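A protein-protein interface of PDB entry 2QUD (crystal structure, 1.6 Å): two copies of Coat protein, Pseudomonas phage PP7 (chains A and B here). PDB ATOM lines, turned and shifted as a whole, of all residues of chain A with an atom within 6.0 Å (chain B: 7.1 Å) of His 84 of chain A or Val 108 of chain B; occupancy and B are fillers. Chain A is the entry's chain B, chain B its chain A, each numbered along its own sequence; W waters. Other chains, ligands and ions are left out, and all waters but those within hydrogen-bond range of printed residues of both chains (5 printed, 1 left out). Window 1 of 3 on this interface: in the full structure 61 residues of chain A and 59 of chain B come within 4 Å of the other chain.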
ATOM      1  N   LEU A  10      15.801  -5.352  27.090  1.00  0.00           N
ATOM      2  CA  LEU A  10      16.379  -6.699  27.030  1.00  0.00           C
ATOM      3  C   LEU A  10      15.931  -7.497  28.257  1.00  0.00           C
ATOM      4  O   LEU A  10      16.055  -7.042  29.387  1.00  0.00           O
ATOM      5  CB  LEU A  10      17.903  -6.618  26.999  1.00  0.00           C
ATOM      6  CG  LEU A  10      18.531  -5.746  25.915  1.00  0.00           C
ATOM      7  CD1 LEU A  10      20.067  -5.865  25.959  1.00  0.00           C
ATOM      8  CD2 LEU A  10      17.968  -6.083  24.540  1.00  0.00           C
ATOM      9  N   VAL A  59      24.798  -2.659   8.765  1.00  0.00           N
ATOM     10  CA  VAL A  59      24.269  -2.397  10.088  1.00  0.00           C
ATOM     11  C   VAL A  59      25.326  -2.817  11.092  1.00  0.00           C
ATOM     12  O   VAL A  59      25.806  -3.940  11.014  1.00  0.00           O
ATOM     13  CB  VAL A  59      22.957  -3.191  10.360  1.00  0.00           C
ATOM     14  CG1 VAL A  59      22.550  -3.116  11.863  1.00  0.00           C
ATOM     15  CG2 VAL A  59      21.818  -2.695   9.460  1.00  0.00           C
ATOM     16  N   ASN A  60      25.716  -1.914  11.998  1.00  0.00           N
ATOM     17  CA  ASN A  60      26.605  -2.294  13.119  1.00  0.00           C
ATOM     18  C   ASN A  60      25.916  -2.088  14.451  1.00  0.00           C
ATOM     19  O   ASN A  60      25.270  -1.079  14.680  1.00  0.00           O
ATOM     20  CB  ASN A  60      27.976  -1.583  13.122  1.00  0.00           C
ATOM     21  CG  ASN A  60      29.008  -2.278  14.068  1.00  0.00           C
ATOM     22  OD1 ASN A  60      29.712  -3.224  13.678  1.00  0.00           O
ATOM     23  ND2 ASN A  60      29.084  -1.812  15.305  1.00  0.00           N
ATOM     24  N   LEU A  61      26.048  -3.079  15.331  1.00  0.00           N
ATOM     25  CA  LEU A  61      25.523  -3.026  16.700  1.00  0.00           C
ATOM     26  C   LEU A  61      26.673  -3.414  17.615  1.00  0.00           C
ATOM     27  O   LEU A  61      27.309  -4.434  17.396  1.00  0.00           O
ATOM     28  CB  LEU A  61      24.376  -4.008  16.908  1.00  0.00           C
ATOM     29  CG  LEU A  61      23.128  -3.863  16.061  1.00  0.00           C
ATOM     30  CD1 LEU A  61      22.147  -4.978  16.444  1.00  0.00           C
ATOM     31  CD2 LEU A  61      22.517  -2.472  16.260  1.00  0.00           C
ATOM     32  N   LYS A  62      26.965  -2.611  18.622  1.00  0.00           N
ATOM     33  CA  LYS A  62      28.073  -2.881  19.525  1.00  0.00           C
ATOM     34  C   LYS A  62      27.581  -2.814  20.960  1.00  0.00           C
ATOM     35  O   LYS A  62      27.199  -1.744  21.430  1.00  0.00           O
ATOM     36  CB  LYS A  62      29.196  -1.856  19.334  1.00  0.00           C
ATOM     37  CG  LYS A  62      30.444  -2.081  20.178  1.00  0.00           C
ATOM     38  CD  LYS A  62      31.432  -0.976  19.840  1.00  0.00           C
ATOM     39  CE  LYS A  62      32.804  -1.177  20.437  1.00  0.00           C
ATOM     40  NZ  LYS A  62      33.538   0.120  20.566  1.00  0.00           N
ATOM     41  N   LEU A  63      27.569  -3.957  21.638  1.00  0.00           N
ATOM     42  CA  LEU A  63      27.186  -4.000  23.051  1.00  0.00           C
ATOM     43  C   LEU A  63      28.463  -4.024  23.866  1.00  0.00           C
ATOM     44  O   LEU A  63      29.277  -4.931  23.743  1.00  0.00           O
ATOM     45  CB  LEU A  63      26.345  -5.235  23.349  1.00  0.00           C
ATOM     46  CG  LEU A  63      25.688  -5.331  24.733  1.00  0.00           C
ATOM     47  CD1 LEU A  63      24.684  -4.198  24.860  1.00  0.00           C
ATOM     48  CD2 LEU A  63      25.037  -6.694  25.001  1.00  0.00           C
ATOM     49  N   TRP A  82      30.424  -7.355  22.460  1.00  0.00           N
ATOM     50  CA  TRP A  82      29.881  -8.209  21.436  1.00  0.00           C
ATOM     51  C   TRP A  82      29.313  -7.315  20.348  1.00  0.00           C
ATOM     52  O   TRP A  82      28.298  -6.640  20.557  1.00  0.00           O
ATOM     53  CB  TRP A  82      28.827  -9.157  21.991  1.00  0.00           C
ATOM     54  CG  TRP A  82      28.415 -10.263  21.039  1.00  0.00           C
ATOM     55  CD1 TRP A  82      28.226 -10.182  19.688  1.00  0.00           C
ATOM     56  CD2 TRP A  82      28.101 -11.607  21.403  1.00  0.00           C
ATOM     57  NE1 TRP A  82      27.797 -11.395  19.193  1.00  0.00           N
ATOM     58  CE2 TRP A  82      27.756 -12.295  20.219  1.00  0.00           C
ATOM     59  CE3 TRP A  82      28.128 -12.312  22.612  1.00  0.00           C
ATOM     60  CZ2 TRP A  82      27.373 -13.626  20.216  1.00  0.00           C
ATOM     61  CZ3 TRP A  82      27.729 -13.634  22.614  1.00  0.00           C
ATOM     62  CH2 TRP A  82      27.370 -14.276  21.429  1.00  0.00           C
ATOM     63  N   SER A  83      30.004  -7.304  19.207  1.00  0.00           N
ATOM     64  CA  SER A  83      29.652  -6.499  18.046  1.00  0.00           C
ATOM     65  C   SER A  83      29.055  -7.345  16.914  1.00  0.00           C
ATOM     66  O   SER A  83      29.444  -8.485  16.745  1.00  0.00           O
ATOM     67  CB  SER A  83      30.890  -5.756  17.513  1.00  0.00           C
ATOM     68  OG  SER A  83      31.307  -4.735  18.403  1.00  0.00           O
ATOM     69  N   HIS A  84      28.144  -6.743  16.158  1.00  0.00           N
ATOM     70  CA  HIS A  84      27.475  -7.335  15.014  1.00  0.00           C
ATOM     71  C   HIS A  84      27.733  -6.471  13.801  1.00  0.00           C
ATOM     72  O   HIS A  84      27.631  -5.255  13.893  1.00  0.00           O
ATOM     73  CB  HIS A  84      25.985  -7.367  15.258  1.00  0.00           C
ATOM     74  CG  HIS A  84      25.614  -8.058  16.528  1.00  0.00           C
ATOM     75  ND1 HIS A  84      25.154  -9.355  16.547  1.00  0.00           N
ATOM     76  CD2 HIS A  84      25.690  -7.662  17.817  1.00  0.00           C
ATOM     77  CE1 HIS A  84      24.951  -9.727  17.799  1.00  0.00           C
ATOM     78  NE2 HIS A  84      25.262  -8.706  18.595  1.00  0.00           N
ATOM     79  N   ASP A  85      28.040  -7.102  12.667  1.00  0.00           N
ATOM     80  CA  ASP A  85      28.194  -6.411  11.390  1.00  0.00           C
ATOM     81  C   ASP A  85      27.324  -7.169  10.410  1.00  0.00           C
ATOM     82  O   ASP A  85      27.630  -8.294  10.063  1.00  0.00           O
ATOM     83  CB  ASP A  85      29.672  -6.384  10.991  1.00  0.00           C
ATOM     84  CG  ASP A  85      29.951  -5.568   9.727  1.00  0.00           C
ATOM     85  OD1 ASP A  85      31.140  -5.285   9.493  1.00  0.00           O
ATOM     86  OD2 ASP A  85      29.023  -5.224   8.972  1.00  0.00           O
ATOM     87  N   VAL A  86      26.231  -6.534   9.992  1.00  0.00           N
ATOM     88  CA  VAL A  86      25.249  -7.151   9.125  1.00  0.00           C
ATOM     89  C   VAL A  86      25.291  -6.495   7.738  1.00  0.00           C
ATOM     90  O   VAL A  86      25.135  -5.283   7.626  1.00  0.00           O
ATOM     91  CB  VAL A  86      23.846  -7.080   9.715  1.00  0.00           C
ATOM     92  CG1 VAL A  86      22.933  -8.043   8.972  1.00  0.00           C
ATOM     93  CG2 VAL A  86      23.869  -7.381  11.209  1.00  0.00           C
ATOM     94  N   TYR A 101      18.174 -13.103   9.671  1.00  0.00           N
ATOM     95  CA  TYR A 101      17.796 -12.780  11.056  1.00  0.00           C
ATOM     96  C   TYR A 101      17.449 -14.037  11.879  1.00  0.00           C
ATOM     97  O   TYR A 101      17.985 -14.261  12.975  1.00  0.00           O
ATOM     98  CB  TYR A 101      16.618 -11.779  11.094  1.00  0.00           C
ATOM     99  CG  TYR A 101      16.109 -11.609  12.499  1.00  0.00           C
ATOM    100  CD1 TYR A 101      16.775 -10.807  13.381  1.00  0.00           C
ATOM    101  CD2 TYR A 101      15.011 -12.298  12.976  1.00  0.00           C
ATOM    102  CE1 TYR A 101      16.405 -10.713  14.692  1.00  0.00           C
ATOM    103  CE2 TYR A 101      14.598 -12.188  14.293  1.00  0.00           C
ATOM    104  CZ  TYR A 101      15.305 -11.404  15.163  1.00  0.00           C
ATOM    105  OH  TYR A 101      14.897 -11.275  16.463  1.00  0.00           O
ATOM    106  N   THR A 104      20.327 -16.283  12.604  1.00  0.00           N
ATOM    107  CA  THR A 104      21.216 -15.696  13.585  1.00  0.00           C
ATOM    108  C   THR A 104      20.681 -15.728  15.006  1.00  0.00           C
ATOM    109  O   THR A 104      21.354 -15.996  15.893  1.00  0.00           O
ATOM    110  CB  THR A 104      21.582 -14.249  13.198  1.00  0.00           C
ATOM    111  OG1 THR A 104      22.223 -14.242  11.944  1.00  0.00           O
ATOM    112  CG2 THR A 104      22.497 -13.656  14.230  1.00  0.00           C
ATOM    113  N   LYS A 105      19.411 -15.412  15.170  1.00  0.00           N
ATOM    114  CA  LYS A 105      18.754 -15.569  16.457  1.00  0.00           C
ATOM    115  C   LYS A 105      18.932 -17.005  16.994  1.00  0.00           C
ATOM    116  O   LYS A 105      19.288 -17.191  18.173  1.00  0.00           O
ATOM    117  CB  LYS A 105      17.276 -15.221  16.311  1.00  0.00           C
ATOM    118  CG  LYS A 105      16.478 -15.359  17.568  1.00  0.00           C
ATOM    119  CD  LYS A 105      15.065 -14.827  17.298  1.00  0.00           C
ATOM    120  CE  LYS A 105      14.129 -15.091  18.441  1.00  0.00           C
ATOM    121  NZ  LYS A 105      12.939 -14.124  18.441  1.00  0.00           N
ATOM    122  N   VAL A 108      22.775 -17.741  17.936  1.00  0.00           N
ATOM    123  CA  VAL A 108      23.208 -17.111  19.195  1.00  0.00           C
ATOM    124  C   VAL A 108      22.600 -17.878  20.364  1.00  0.00           C
ATOM    125  O   VAL A 108      23.256 -18.049  21.379  1.00  0.00           O
ATOM    126  CB  VAL A 108      22.908 -15.568  19.222  1.00  0.00           C
ATOM    127  CG1 VAL A 108      23.191 -14.991  20.601  1.00  0.00           C
ATOM    128  CG2 VAL A 108      23.706 -14.862  18.110  1.00  0.00           C
ATOM    129  N   TRP B  82      25.917 -11.946   8.366  1.00  0.00           N
ATOM    130  CA  TRP B  82      25.871 -11.456   9.731  1.00  0.00           C
ATOM    131  C   TRP B  82      27.029 -11.972  10.524  1.00  0.00           C
ATOM    132  O   TRP B  82      27.115 -13.128  10.808  1.00  0.00           O
ATOM    133  CB  TRP B  82      24.549 -11.812  10.379  1.00  0.00           C
ATOM    134  CG  TRP B  82      24.224 -11.165  11.696  1.00  0.00           C
ATOM    135  CD1 TRP B  82      25.076 -10.874  12.716  1.00  0.00           C
ATOM    136  CD2 TRP B  82      22.936 -10.763  12.136  1.00  0.00           C
ATOM    137  NE1 TRP B  82      24.403 -10.319  13.743  1.00  0.00           N
ATOM    138  CE2 TRP B  82      23.080 -10.245  13.423  1.00  0.00           C
ATOM    139  CE3 TRP B  82      21.667 -10.822  11.578  1.00  0.00           C
ATOM    140  CZ2 TRP B  82      22.001  -9.769  14.139  1.00  0.00           C
ATOM    141  CZ3 TRP B  82      20.639 -10.356  12.263  1.00  0.00           C
ATOM    142  CH2 TRP B  82      20.788  -9.816  13.524  1.00  0.00           C
ATOM    143  N   SER B  83      27.932 -11.063  10.844  1.00  0.00           N
ATOM    144  CA  SER B  83      29.123 -11.465  11.560  1.00  0.00           C
ATOM    145  C   SER B  83      29.124 -10.916  12.986  1.00  0.00           C
ATOM    146  O   SER B  83      28.511  -9.907  13.287  1.00  0.00           O
ATOM    147  CB  SER B  83      30.392 -11.065  10.805  1.00  0.00           C
ATOM    148  OG  SER B  83      30.444  -9.673  10.639  1.00  0.00           O
ATOM    149  N   HIS B  84      29.814 -11.643  13.844  1.00  0.00           N
ATOM    150  CA  HIS B  84      29.960 -11.374  15.272  1.00  0.00           C
ATOM    151  C   HIS B  84      31.416 -11.227  15.595  1.00  0.00           C
ATOM    152  O   HIS B  84      32.247 -11.984  15.112  1.00  0.00           O
ATOM    153  CB  HIS B  84      29.378 -12.521  16.107  1.00  0.00           C
ATOM    154  CG  HIS B  84      27.975 -12.851  15.749  1.00  0.00           C
ATOM    155  ND1 HIS B  84      26.884 -12.418  16.474  1.00  0.00           N
ATOM    156  CD2 HIS B  84      27.482 -13.545  14.701  1.00  0.00           C
ATOM    157  CE1 HIS B  84      25.779 -12.842  15.884  1.00  0.00           C
ATOM    158  NE2 HIS B  84      26.114 -13.527  14.802  1.00  0.00           N
ATOM    159  N   ASP B  85      31.729 -10.257  16.454  1.00  0.00           N
ATOM    160  CA  ASP B  85      33.087 -10.050  16.929  1.00  0.00           C
ATOM    161  C   ASP B  85      32.930  -9.875  18.436  1.00  0.00           C
ATOM    162  O   ASP B  85      32.370  -8.887  18.892  1.00  0.00           O
ATOM    163  CB  ASP B  85      33.676  -8.824  16.273  1.00  0.00           C
ATOM    164  CG  ASP B  85      35.157  -8.666  16.525  1.00  0.00           C
ATOM    165  OD1 ASP B  85      35.835  -8.276  15.561  1.00  0.00           O
ATOM    166  OD2 ASP B  85      35.650  -8.912  17.642  1.00  0.00           O
ATOM    167  N   LEU B 103      22.679 -11.155  27.453  1.00  0.00           N
ATOM    168  CA  LEU B 103      22.189  -9.874  26.915  1.00  0.00           C
ATOM    169  C   LEU B 103      22.197  -9.844  25.384  1.00  0.00           C
ATOM    170  O   LEU B 103      21.288  -9.282  24.767  1.00  0.00           O
ATOM    171  CB  LEU B 103      23.010  -8.717  27.466  1.00  0.00           C
ATOM    172  CG  LEU B 103      22.786  -8.473  28.971  1.00  0.00           C
ATOM    173  CD1 LEU B 103      23.927  -7.592  29.514  1.00  0.00           C
ATOM    174  CD2 LEU B 103      21.444  -7.783  29.259  1.00  0.00           C
ATOM    175  N   THR B 104      23.201 -10.437  24.764  1.00  0.00           N
ATOM    176  CA  THR B 104      23.250 -10.455  23.323  1.00  0.00           C
ATOM    177  C   THR B 104      22.163 -11.371  22.740  1.00  0.00           C
ATOM    178  O   THR B 104      21.567 -11.051  21.827  1.00  0.00           O
ATOM    179  CB  THR B 104      24.603 -10.900  22.810  1.00  0.00           C
ATOM    180  OG1 THR B 104      25.581  -9.970  23.221  1.00  0.00           O
ATOM    181  CG2 THR B 104      24.595 -10.991  21.333  1.00  0.00           C
ATOM    182  N   LYS B 105      21.967 -12.526  23.342  1.00  0.00           N
ATOM    183  CA  LYS B 105      20.880 -13.416  22.974  1.00  0.00           C
ATOM    184  C   LYS B 105      19.561 -12.666  23.018  1.00  0.00           C
ATOM    185  O   LYS B 105      18.804 -12.741  22.051  1.00  0.00           O
ATOM    186  CB  LYS B 105      20.869 -14.685  23.846  1.00  0.00           C
ATOM    187  CG  LYS B 105      19.729 -15.647  23.591  1.00  0.00           C
ATOM    188  CD  LYS B 105      19.772 -16.766  24.608  1.00  0.00           C
ATOM    189  CE  LYS B 105      18.637 -17.787  24.399  1.00  0.00           C
ATOM    190  NZ  LYS B 105      17.246 -17.220  24.336  1.00  0.00           N
ATOM    191  N   SER B 106      19.327 -11.919  24.104  1.00  0.00           N
ATOM    192  CA  SER B 106      18.117 -11.101  24.239  1.00  0.00           C
ATOM    193  C   SER B 106      18.025 -10.007  23.181  1.00  0.00           C
ATOM    194  O   SER B 106      16.987  -9.854  22.532  1.00  0.00           O
ATOM    195  CB  SER B 106      18.030 -10.475  25.623  1.00  0.00           C
ATOM    196  OG  SER B 106      16.790  -9.823  25.788  1.00  0.00           O
ATOM    197  N   LEU B 107      19.113  -9.258  22.994  1.00  0.00           N
ATOM    198  CA  LEU B 107      19.139  -8.217  21.974  1.00  0.00           C
ATOM    199  C   LEU B 107      18.760  -8.709  20.585  1.00  0.00           C
ATOM    200  O   LEU B 107      17.892  -8.133  19.943  1.00  0.00           O
ATOM    201  CB  LEU B 107      20.528  -7.604  21.933  1.00  0.00           C
ATOM    202  CG  LEU B 107      20.875  -6.496  20.909  1.00  0.00           C
ATOM    203  CD1 LEU B 107      19.945  -5.265  21.086  1.00  0.00           C
ATOM    204  CD2 LEU B 107      22.360  -6.144  21.003  1.00  0.00           C
ATOM    205  N   VAL B 108      19.418  -9.769  20.131  1.00  0.00           N
ATOM    206  CA  VAL B 108      19.175 -10.333  18.816  1.00  0.00           C
ATOM    207  C   VAL B 108      17.731 -10.775  18.698  1.00  0.00           C
ATOM    208  O   VAL B 108      17.120 -10.562  17.670  1.00  0.00           O
ATOM    209  CB  VAL B 108      20.145 -11.491  18.500  1.00  0.00           C
ATOM    210  CG1 VAL B 108      19.759 -12.155  17.174  1.00  0.00           C
ATOM    211  CG2 VAL B 108      21.551 -10.972  18.435  1.00  0.00           C
ATOM    212  N   ALA B 109      17.196 -11.357  19.774  1.00  0.00           N
ATOM    213  CA  ALA B 109      15.811 -11.848  19.794  1.00  0.00           C
ATOM    214  C   ALA B 109      14.746 -10.753  19.757  1.00  0.00           C
ATOM    215  O   ALA B 109      13.578 -11.068  19.481  1.00  0.00           O
ATOM    216  CB  ALA B 109      15.586 -12.751  20.990  1.00  0.00           C
ATOM    217  N   THR B 110      15.096  -9.489  20.023  1.00  0.00           N
ATOM    218  CA  THR B 110      14.111  -8.400  20.001  1.00  0.00           C
ATOM    219  C   THR B 110      13.448  -8.168  18.634  1.00  0.00           C
ATOM    220  O   THR B 110      14.079  -8.288  17.571  1.00  0.00           O
ATOM    221  CB  THR B 110      14.704  -7.038  20.501  1.00  0.00           C
ATOM    222  OG1 THR B 110      15.724  -6.552  19.621  1.00  0.00           O
ATOM    223  CG2 THR B 110      15.214  -7.163  21.933  1.00  0.00           C
ATOM    224  N   SER B 111      12.158  -7.827  18.667  1.00  0.00           N
ATOM    225  CA  SER B 111      11.471  -7.417  17.439  1.00  0.00           C
ATOM    226  C   SER B 111      12.098  -6.156  16.836  1.00  0.00           C
ATOM    227  O   SER B 111      12.084  -5.991  15.605  1.00  0.00           O
ATOM    228  CB  SER B 111       9.961  -7.254  17.668  1.00  0.00           C
ATOM    229  OG  SER B 111       9.714  -6.384  18.735  1.00  0.00           O
ATOM    230  N   GLN B 112      12.675  -5.290  17.678  1.00  0.00           N
ATOM    231  CA  GLN B 112      13.404  -4.109  17.192  1.00  0.00           C
ATOM    232  C   GLN B 112      14.598  -4.438  16.292  1.00  0.00           C
ATOM    233  O   GLN B 112      14.711  -3.883  15.202  1.00  0.00           O
ATOM    234  CB  GLN B 112      13.860  -3.227  18.361  1.00  0.00           C
ATOM    235  CG  GLN B 112      12.738  -2.466  19.038  1.00  0.00           C
ATOM    236  CD  GLN B 112      13.231  -1.405  20.010  1.00  0.00           C
ATOM    237  OE1 GLN B 112      14.264  -0.780  19.780  1.00  0.00           O
ATOM    238  NE2 GLN B 112      12.476  -1.191  21.096  1.00  0.00           N
ATOM    239  N   VAL B 113      15.471  -5.355  16.717  1.00  0.00           N
ATOM    240  CA  VAL B 113      16.602  -5.779  15.876  1.00  0.00           C
ATOM    241  C   VAL B 113      16.098  -6.452  14.588  1.00  0.00           C
ATOM    242  O   VAL B 113      16.627  -6.249  13.514  1.00  0.00           O
ATOM    243  CB  VAL B 113      17.569  -6.689  16.669  1.00  0.00           C
ATOM    244  CG1 VAL B 113      18.593  -7.364  15.725  1.00  0.00           C
ATOM    245  CG2 VAL B 113      18.280  -5.869  17.749  1.00  0.00           C
ATOM    246  N   GLU B 114      15.032  -7.245  14.712  1.00  0.00           N
ATOM    247  CA  GLU B 114      14.422  -7.871  13.548  1.00  0.00           C
ATOM    248  C   GLU B 114      14.017  -6.795  12.527  1.00  0.00           C
ATOM    249  O   GLU B 114      14.268  -6.934  11.345  1.00  0.00           O
ATOM    250  CB  GLU B 114      13.191  -8.717  13.922  1.00  0.00           C
ATOM    251  CG  GLU B 114      12.650  -9.524  12.737  1.00  0.00           C
ATOM    252  CD  GLU B 114      11.498 -10.443  13.063  1.00  0.00           C
ATOM    253  OE1 GLU B 114      11.179 -10.627  14.252  1.00  0.00           O
ATOM    254  OE2 GLU B 114      10.900 -10.986  12.104  1.00  0.00           O
HETATM  255  O   HOH W   1      30.992  -7.919  13.973  1.00  0.00           O
HETATM  256  O   HOH W   2      25.660  -7.868  21.234  1.00  0.00           O
HETATM  257  O   HOH W   3      18.720 -15.157  20.321  1.00  0.00           O
HETATM  258  O   HOH W   4      25.100 -14.651  12.429  1.00  0.00           O
HETATM  259  O   HOH W   5      32.758  -7.867   9.696  1.00  0.00           O
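The side-chain amide oxygen of Asn 60 of chain A lies close to the backbone carbonyl oxygen of His 84 of chain A (2.9 Å).
O of Leu 61 of chain A is in hydrogen-bond range of N of His 84 of chain A.
The backbone NH (N) of Trp 82 of chain A sits at hydrogen-bond distance from the backbone carbonyl oxygen (O) of Leu 63 of chain A (3.0 Å).
The backbone NH (N) of Val 113 of chain B is in hydrogen-bond range of the side-chain hydroxyl (OG1) of Thr 110 of chain B (3.2 Å).
O of Leu 107 of chain B sits at hydrogen-bond distance from OG1 of Thr 110 of chain B, at 2.7 Å.
O of Val 59 of chain A is in hydrogen-bond range of N of Val 86 of chain A (2.8 Å).
Water W2 lies within hydrogen-bond range of a ring nitrogen (NE2) of His 84 of chain A (2.8 Å), the side-chain hydroxyl of Thr 104 of chain B (2.9 Å) and the backbone carbonyl oxygen of Trp 82 of chain A (3.0 Å).
Water W4 lies within hydrogen-bond range of NE2 of His 84 of chain B (2.8 Å), OG1 of Thr 104 of chain A (2.9 Å) and O of Trp 82 of chain B (3.0 Å).
Water W3 lies within hydrogen-bond range of O of Lys 105 of chain B and O of Lys 105 of chain A.
Water W5 bridges OD1 of Asp 85 of chain A (3.1 Å) and OG of Ser 83 of chain B (3.1 Å).
Water W1 lies within hydrogen-bond range of O of Ser 83 of chain A (3.2 Å), O of Ser 83 of chain B (3.3 Å), N of Asp 85 of chain A (3.3 Å) and N of Asp 85 of chain B (3.5 Å).
Among the printed residues, merely in contact across the chains: His 84 of chain A with Ser 83 of chain B, Ser 83 of chain A with His 84 of chain B, Leu 10 of chain A with Ser 106 of chain B, Thr 104 of chain A with Trp 82 of chain B, Trp 82 of chain A with Thr 104 of chain B, His 84 of chain A with His 84 of chain B, Leu 10 of chain A with Leu 107 of chain B, Trp 82 of chain A with Asp 85 of chain B, His 84 of chain A with Thr 104 of chain B, Val 86 of chain A with Trp 82 of chain B, Lys 105 of chain A with Val 108 of chain B, Asp 85 of chain A with Trp 82 of chain B, Tyr 101 of chain A with Glu 114 of chain B, Val 108 of chain A with His 84 of chain B, Thr 104 of chain A with His 84 of chain B, Val 108 of chain A with Lys 105 of chain B, His 84 of chain A with Val 108 of chain B, Leu 63 of chain A with Thr 104 of chain B, Leu 63 of chain A with Leu 103 of chain B, Leu 10 of chain A with Leu 103 of chain B, Ser 83 of chain A with Ser 83 of chain B, Tyr 101 of chain A with Trp 82 of chain B and Leu 10 of chain A with Thr 110 of chain B.
Of the printed residues of chain B, His 84 of chain A touches Trp 82 (3.1 Å), Ser 83 (3.3 Å), His 84 (3.5 Å), Thr 104 (3.6 Å) and Val 108 (3.7 Å).
Val 108 of chain B touches just these residues of chain A: His 84, Tyr 101 and Lys 105.
Printed residues of chain A within 4 Å of Trp 82 of chain B: His 84 (3.1 Å), Asp 85 (3.6 Å), Val 86 (3.6 Å), Tyr 101 (3.9 Å) and Thr 104 (3.5 Å).
Of the printed residues of chain B, Leu 63 of chain A touches Leu 103 and Thr 104.
Printed residues of chain B within 4 Å of Ser 83 of chain A: Ser 83 (3.9 Å), His 84 (3.3 Å) and Asp 85 (2.9 Å).
Gln 112 of chain B touches none of the printed residues of chain A.
The nearest printed residue of chain B that does not touch His 84 of chain A is Leu 107 of chain B (4.6 Å).
The nearest residue of chain A that does not touch Val 108 of chain B is Thr 104 of chain A (4.3 Å).
The nearest printed residue of chain B that does not touch Asp 85 of chain A is His 84 of chain B (5.0 Å).
Trp 82 of chain A touches His 84 of chain B, and with the chains exchanged His 84 of chain A touches Trp 82 of chain B.
Ser 83 of chain A touches His 84 of chain B, and with the chains exchanged His 84 of chain A touches Ser 83 of chain B.
Ser 83 of chain A touches Asp 85 of chain B, and with the chains exchanged Asp 85 of chain A touches Ser 83 of chain B.
Lys 105 of chain A touches Val 108 of chain B, and with the chains exchanged Val 108 of chain A touches Lys 105 of chain B.
Of the 31 pairs that touch across the chains among the printed residues, 18 have their exchanged pair printed and touching as well.
Printed residues of chain A that touch a printed residue of chain B: Leu 10, Leu 63, Trp 82, Ser 83, His 84, Asp 85, Val 86, Tyr 101, Thr 104, Lys 105 and Val 108.
Hydrophobic or aromatic side chains of chain A within 4 Å of the printed part of chain B: Leu 10, Leu 63, Trp 82, His 84, Val 86, Tyr 101 and Val 108.
Among the printed residues, 31 pairs touch across the chains.
Among the printed residues, no Asp or Glu carboxylate lies within 4 Å of a Lys or Arg side-chain nitrogen of the other chain.
The backbone carbonyl oxygen of Asp 85 of chain B lies within hydrogen-bond range of the backbone NH of Ser 83 of chain A, 2.9 Å away.
The side-chain hydroxyl (OH) of Tyr 101 of chain A sits at hydrogen-bond distance from the backbone carbonyl oxygen (O) of Thr 110 of chain B (3.3 Å).
ND1 of His 84 of chain B is in hydrogen-bond range of NE1 of Trp 82 of chain A (3.0 Å).
O of Ala 109 of chain B lies within hydrogen-bond range of OH of Tyr 101 of chain A.
NE1 of Trp 82 of chain B is in hydrogen-bond range of ND1 of His 84 of chain A (3.1 Å).
N of Ser 83 of chain B sits at hydrogen-bond distance from O of Asp 85 of chain A (2.9 Å).
The backbone carbonyl oxygen (O) of Ala 109 of chain B lies within hydrogen-bond range of the side-chain amino group (NZ) of Lys 105 of chain A, at 3.3 Å.
O of Val 108 of chain B sits at hydrogen-bond distance from OH of Tyr 101 of chain A, 2.6 Å away.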
